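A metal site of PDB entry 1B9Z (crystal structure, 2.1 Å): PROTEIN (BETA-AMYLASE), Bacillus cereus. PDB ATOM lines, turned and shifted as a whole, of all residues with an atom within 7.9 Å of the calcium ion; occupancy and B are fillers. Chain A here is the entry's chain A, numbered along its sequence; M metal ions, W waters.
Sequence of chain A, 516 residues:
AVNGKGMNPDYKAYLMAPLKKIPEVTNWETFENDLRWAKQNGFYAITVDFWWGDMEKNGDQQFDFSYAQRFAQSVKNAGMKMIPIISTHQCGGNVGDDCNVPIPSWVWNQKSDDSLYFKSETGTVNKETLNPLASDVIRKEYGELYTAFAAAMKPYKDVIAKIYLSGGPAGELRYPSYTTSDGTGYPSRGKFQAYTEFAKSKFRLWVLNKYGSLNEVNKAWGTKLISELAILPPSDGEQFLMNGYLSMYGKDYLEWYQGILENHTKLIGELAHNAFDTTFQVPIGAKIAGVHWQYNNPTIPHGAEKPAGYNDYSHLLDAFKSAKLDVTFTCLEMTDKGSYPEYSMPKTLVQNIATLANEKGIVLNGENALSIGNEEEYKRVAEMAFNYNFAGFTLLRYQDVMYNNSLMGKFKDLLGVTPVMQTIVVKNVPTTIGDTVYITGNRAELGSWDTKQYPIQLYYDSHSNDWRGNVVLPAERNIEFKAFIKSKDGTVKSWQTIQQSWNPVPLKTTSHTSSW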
ATOM      1  N   TRP A  52       8.284 -18.286  20.587  1.00  0.00           N
ATOM      2  CA  TRP A  52       8.622 -17.080  19.833  1.00  0.00           C
ATOM      3  C   TRP A  52       7.985 -17.130  18.455  1.00  0.00           C
ATOM      4  O   TRP A  52       7.527 -16.119  17.924  1.00  0.00           O
ATOM      5  CB  TRP A  52      10.154 -16.963  19.684  1.00  0.00           C
ATOM      6  CG  TRP A  52      10.676 -15.590  19.218  1.00  0.00           C
ATOM      7  CD1 TRP A  52       9.868 -14.479  19.165  1.00  0.00           C
ATOM      8  CD2 TRP A  52      11.959 -15.311  18.793  1.00  0.00           C
ATOM      9  NE1 TRP A  52      10.609 -13.508  18.703  1.00  0.00           N
ATOM     10  CE2 TRP A  52      11.855 -13.941  18.454  1.00  0.00           C
ATOM     11  CE3 TRP A  52      13.174 -15.990  18.622  1.00  0.00           C
ATOM     12  CZ2 TRP A  52      12.945 -13.225  17.960  1.00  0.00           C
ATOM     13  CZ3 TRP A  52      14.267 -15.268  18.115  1.00  0.00           C
ATOM     14  CH2 TRP A  52      14.148 -13.910  17.792  1.00  0.00           C
ATOM     15  N   GLU A  56       5.550 -13.505  17.601  1.00  0.00           N
ATOM     16  CA  GLU A  56       6.096 -12.510  16.700  1.00  0.00           C
ATOM     17  C   GLU A  56       6.377 -13.209  15.392  1.00  0.00           C
ATOM     18  O   GLU A  56       7.420 -13.045  14.764  1.00  0.00           O
ATOM     19  CB  GLU A  56       7.378 -11.938  17.321  1.00  0.00           C
ATOM     20  CG  GLU A  56       7.991 -10.750  16.565  1.00  0.00           C
ATOM     21  CD  GLU A  56       9.233 -10.096  17.176  1.00  0.00           C
ATOM     22  OE1 GLU A  56       9.824 -10.614  18.111  1.00  0.00           O
ATOM     23  OE2 GLU A  56       9.614  -9.027  16.710  1.00  0.00           O
ATOM     24  N   GLY A  59       6.342 -10.633  11.346  1.00  0.00           N
ATOM     25  CA  GLY A  59       7.406  -9.710  11.055  1.00  0.00           C
ATOM     26  C   GLY A  59       7.890  -9.108  12.346  1.00  0.00           C
ATOM     27  O   GLY A  59       7.293  -9.267  13.420  1.00  0.00           O
ATOM     28  N   ASP A  60       8.989  -8.374  12.212  1.00  0.00           N
ATOM     29  CA  ASP A  60       9.612  -7.709  13.334  1.00  0.00           C
ATOM     30  C   ASP A  60       8.650  -6.669  13.843  1.00  0.00           C
ATOM     31  O   ASP A  60       8.041  -5.899  13.085  1.00  0.00           O
ATOM     32  CB  ASP A  60      10.927  -7.103  12.839  1.00  0.00           C
ATOM     33  CG  ASP A  60      11.844  -6.617  13.943  1.00  0.00           C
ATOM     34  OD1 ASP A  60      11.777  -7.088  15.078  1.00  0.00           O
ATOM     35  OD2 ASP A  60      12.639  -5.741  13.640  1.00  0.00           O
ATOM     36  N   GLN A  61       8.551  -6.717  15.168  1.00  0.00           N
ATOM     37  CA  GLN A  61       7.677  -5.863  15.944  1.00  0.00           C
ATOM     38  C   GLN A  61       6.190  -6.099  15.705  1.00  0.00           C
ATOM     39  O   GLN A  61       5.381  -5.315  16.192  1.00  0.00           O
ATOM     40  CB  GLN A  61       7.962  -4.365  15.706  1.00  0.00           C
ATOM     41  CG  GLN A  61       9.332  -3.901  16.193  1.00  0.00           C
ATOM     42  CD  GLN A  61       9.661  -4.291  17.630  1.00  0.00           C
ATOM     43  OE1 GLN A  61      10.052  -5.448  17.886  1.00  0.00           O
ATOM     44  NE2 GLN A  61       9.536  -3.374  18.605  1.00  0.00           N
ATOM     45  N   GLN A  62       5.796  -7.149  14.949  1.00  0.00           N
ATOM     46  CA  GLN A  62       4.372  -7.443  14.721  1.00  0.00           C
ATOM     47  C   GLN A  62       4.000  -8.532  15.737  1.00  0.00           C
ATOM     48  O   GLN A  62       4.039  -9.712  15.417  1.00  0.00           O
ATOM     49  CB  GLN A  62       4.204  -7.926  13.278  1.00  0.00           C
ATOM     50  CG  GLN A  62       4.213  -6.769  12.268  1.00  0.00           C
ATOM     51  CD  GLN A  62       4.378  -7.186  10.803  1.00  0.00           C
ATOM     52  OE1 GLN A  62       5.393  -6.886  10.168  1.00  0.00           O
ATOM     53  NE2 GLN A  62       3.373  -7.870  10.240  1.00  0.00           N
ATOM     54  N   PHE A  63       3.717  -8.150  16.983  1.00  0.00           N
ATOM     55  CA  PHE A  63       3.385  -9.011  18.116  1.00  0.00           C
ATOM     56  C   PHE A  63       1.929  -9.426  18.389  1.00  0.00           C
ATOM     57  O   PHE A  63       0.966  -8.660  18.235  1.00  0.00           O
ATOM     58  CB  PHE A  63       3.905  -8.373  19.424  1.00  0.00           C
ATOM     59  CG  PHE A  63       5.384  -7.984  19.534  1.00  0.00           C
ATOM     60  CD1 PHE A  63       6.399  -8.964  19.631  1.00  0.00           C
ATOM     61  CD2 PHE A  63       5.755  -6.629  19.518  1.00  0.00           C
ATOM     62  CE1 PHE A  63       7.741  -8.591  19.718  1.00  0.00           C
ATOM     63  CE2 PHE A  63       7.102  -6.269  19.609  1.00  0.00           C
ATOM     64  CZ  PHE A  63       8.095  -7.250  19.709  1.00  0.00           C
ATOM     65  N   TRP A 106      11.648 -14.891   9.381  1.00  0.00           N
ATOM     66  CA  TRP A 106      12.224 -13.611   9.042  1.00  0.00           C
ATOM     67  C   TRP A 106      13.490 -13.269   9.839  1.00  0.00           C
ATOM     68  O   TRP A 106      14.249 -12.379   9.431  1.00  0.00           O
ATOM     69  CB  TRP A 106      11.162 -12.489   9.264  1.00  0.00           C
ATOM     70  CG  TRP A 106      10.614 -12.361  10.666  1.00  0.00           C
ATOM     71  CD1 TRP A 106       9.408 -12.929  10.980  1.00  0.00           C
ATOM     72  CD2 TRP A 106      11.214 -11.754  11.755  1.00  0.00           C
ATOM     73  NE1 TRP A 106       9.224 -12.693  12.261  1.00  0.00           N
ATOM     74  CE2 TRP A 106      10.263 -12.009  12.768  1.00  0.00           C
ATOM     75  CE3 TRP A 106      12.387 -11.049  12.063  1.00  0.00           C
ATOM     76  CZ2 TRP A 106      10.473 -11.587  14.088  1.00  0.00           C
ATOM     77  CZ3 TRP A 106      12.601 -10.618  13.381  1.00  0.00           C
ATOM     78  CH2 TRP A 106      11.644 -10.887  14.377  1.00  0.00           C
ATOM     79  N   GLN A 110      17.957 -11.292   8.474  1.00  0.00           N
ATOM     80  CA  GLN A 110      18.587 -10.062   8.953  1.00  0.00           C
ATOM     81  C   GLN A 110      20.085  -9.981   8.723  1.00  0.00           C
ATOM     82  O   GLN A 110      20.651  -8.917   8.975  1.00  0.00           O
ATOM     83  CB  GLN A 110      18.329  -9.887  10.427  1.00  0.00           C
ATOM     84  CG  GLN A 110      16.894  -9.536  10.729  1.00  0.00           C
ATOM     85  CD  GLN A 110      16.834  -8.535  11.861  1.00  0.00           C
ATOM     86  OE1 GLN A 110      16.010  -7.614  11.836  1.00  0.00           O
ATOM     87  NE2 GLN A 110      17.692  -8.653  12.901  1.00  0.00           N
ATOM     88  N   VAL A 137      22.246  -9.129  17.197  1.00  0.00           N
ATOM     89  CA  VAL A 137      20.920  -9.485  16.778  1.00  0.00           C
ATOM     90  C   VAL A 137      20.238  -9.934  18.064  1.00  0.00           C
ATOM     91  O   VAL A 137      19.075  -9.590  18.257  1.00  0.00           O
ATOM     92  CB  VAL A 137      20.986 -10.618  15.769  1.00  0.00           C
ATOM     93  CG1 VAL A 137      19.610 -11.234  15.528  1.00  0.00           C
ATOM     94  CG2 VAL A 137      21.509 -10.059  14.467  1.00  0.00           C
ATOM     95  N   LYS A 140      19.185  -6.913  20.220  1.00  0.00           N
ATOM     96  CA  LYS A 140      18.066  -6.237  19.575  1.00  0.00           C
ATOM     97  C   LYS A 140      16.763  -7.039  19.718  1.00  0.00           C
ATOM     98  O   LYS A 140      15.836  -6.572  20.364  1.00  0.00           O
ATOM     99  CB  LYS A 140      18.373  -6.041  18.110  1.00  0.00           C
ATOM    100  CG  LYS A 140      17.202  -5.390  17.361  1.00  0.00           C
ATOM    101  CD  LYS A 140      17.383  -5.518  15.860  1.00  0.00           C
ATOM    102  CE  LYS A 140      16.231  -4.850  15.115  1.00  0.00           C
ATOM    103  NZ  LYS A 140      14.975  -5.566  15.301  1.00  0.00           N
ATOM    104  N   GLU A 141      16.666  -8.246  19.147  1.00  0.00           N
ATOM    105  CA  GLU A 141      15.464  -9.049  19.217  1.00  0.00           C
ATOM    106  C   GLU A 141      14.982  -9.508  20.558  1.00  0.00           C
ATOM    107  O   GLU A 141      13.780  -9.406  20.797  1.00  0.00           O
ATOM    108  CB  GLU A 141      15.605 -10.277  18.355  1.00  0.00           C
ATOM    109  CG  GLU A 141      15.974 -10.063  16.889  1.00  0.00           C
ATOM    110  CD  GLU A 141      15.154  -9.021  16.155  1.00  0.00           C
ATOM    111  OE1 GLU A 141      13.973  -8.815  16.455  1.00  0.00           O
ATOM    112  OE2 GLU A 141      15.725  -8.401  15.260  1.00  0.00           O
ATOM    113  N   TYR A 142      15.841 -10.013  21.473  1.00  0.00           N
ATOM    114  CA  TYR A 142      15.382 -10.474  22.770  1.00  0.00           C
ATOM    115  C   TYR A 142      14.994  -9.270  23.549  1.00  0.00           C
ATOM    116  O   TYR A 142      14.008  -9.316  24.293  1.00  0.00           O
ATOM    117  CB  TYR A 142      16.439 -11.209  23.598  1.00  0.00           C
ATOM    118  CG  TYR A 142      16.742 -12.641  23.179  1.00  0.00           C
ATOM    119  CD1 TYR A 142      16.547 -13.028  21.847  1.00  0.00           C
ATOM    120  CD2 TYR A 142      17.289 -13.573  24.086  1.00  0.00           C
ATOM    121  CE1 TYR A 142      16.879 -14.317  21.414  1.00  0.00           C
ATOM    122  CE2 TYR A 142      17.623 -14.880  23.669  1.00  0.00           C
ATOM    123  CZ  TYR A 142      17.425 -15.251  22.311  1.00  0.00           C
ATOM    124  OH  TYR A 142      17.782 -16.512  21.794  1.00  0.00           O
ATOM    125  N   GLY A 143      15.757  -8.176  23.405  1.00  0.00           N
ATOM    126  CA  GLY A 143      15.437  -6.945  24.116  1.00  0.00           C
ATOM    127  C   GLY A 143      13.999  -6.483  23.840  1.00  0.00           C
ATOM    128  O   GLY A 143      13.263  -6.213  24.788  1.00  0.00           O
ATOM    129  N   GLU A 144      13.598  -6.432  22.554  1.00  0.00           N
ATOM    130  CA  GLU A 144      12.265  -6.016  22.113  1.00  0.00           C
ATOM    131  C   GLU A 144      11.207  -6.989  22.566  1.00  0.00           C
ATOM    132  O   GLU A 144      10.179  -6.539  23.070  1.00  0.00           O
ATOM    133  CB  GLU A 144      12.154  -5.961  20.607  1.00  0.00           C
ATOM    134  CG  GLU A 144      13.085  -4.908  20.059  1.00  0.00           C
ATOM    135  CD  GLU A 144      13.280  -4.953  18.552  1.00  0.00           C
ATOM    136  OE1 GLU A 144      13.108  -6.007  17.932  1.00  0.00           O
ATOM    137  OE2 GLU A 144      13.629  -3.913  17.994  1.00  0.00           O
ATOM    138  N   LEU A 145      11.496  -8.312  22.410  1.00  0.00           N
ATOM    139  CA  LEU A 145      10.549  -9.336  22.825  1.00  0.00           C
ATOM    140  C   LEU A 145      10.339  -9.302  24.316  1.00  0.00           C
ATOM    141  O   LEU A 145       9.189  -9.348  24.688  1.00  0.00           O
ATOM    142  CB  LEU A 145      11.010 -10.753  22.449  1.00  0.00           C
ATOM    143  CG  LEU A 145       9.954 -11.861  22.712  1.00  0.00           C
ATOM    144  CD1 LEU A 145       8.718 -11.573  21.891  1.00  0.00           C
ATOM    145  CD2 LEU A 145      10.524 -13.225  22.362  1.00  0.00           C
HETATM  146 CA    CA M   1      11.867  -7.587  17.191  1.00  0.00          CA
HETATM  147  O   HOH W   1      11.600  -8.957  19.184  1.00  0.00           O
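Water W1 lies within hydrogen-bond range of OE1 of Glu 56 (2.7 Å), O of Glu 141 (2.7 Å) and N of Leu 145 (3.3 Å).
Within 4 Å of the calcium ion: Glu 56, Asp 60, Gln 61, Glu 141 and Glu 144.
OE1 of Glu 144 is bound to the calcium ion (2.1 Å).
OD1 of Asp 60 is bound to the calcium ion.
Water W1 is bound to the calcium ion (2.4 Å).
OE1 of Glu 141 binds the calcium ion (2.5 Å).
The side-chain carboxylate (OE2) of Glu 56 binds the calcium ion (2.7 Å).
OE1 of Gln 61 is bound to the calcium ion, at 2.9 Å.
OE2 of Glu 144 is in salt-bridge range of NZ of Lys 140, 3.4 Å away.
OD2 of Asp 60 is in salt-bridge range of NZ of Lys 140 (2.9 Å).
NZ of Lys 140 lies within salt-bridge range of OE2 of Glu 141 (2.9 Å).
The side-chain amide nitrogen (NE2) of Gln 110 is in hydrogen-bond range of the side-chain carboxylate (OE2) of Glu 141, 3.1 Å away.
NE1 of Trp 106 is in hydrogen-bond range of O of Glu 56, at 3.1 Å.
The side-chain carboxylate (OE1) of Glu 56 is in hydrogen-bond range of the indole nitrogen (NE1) of Trp 52, 3.1 Å away.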
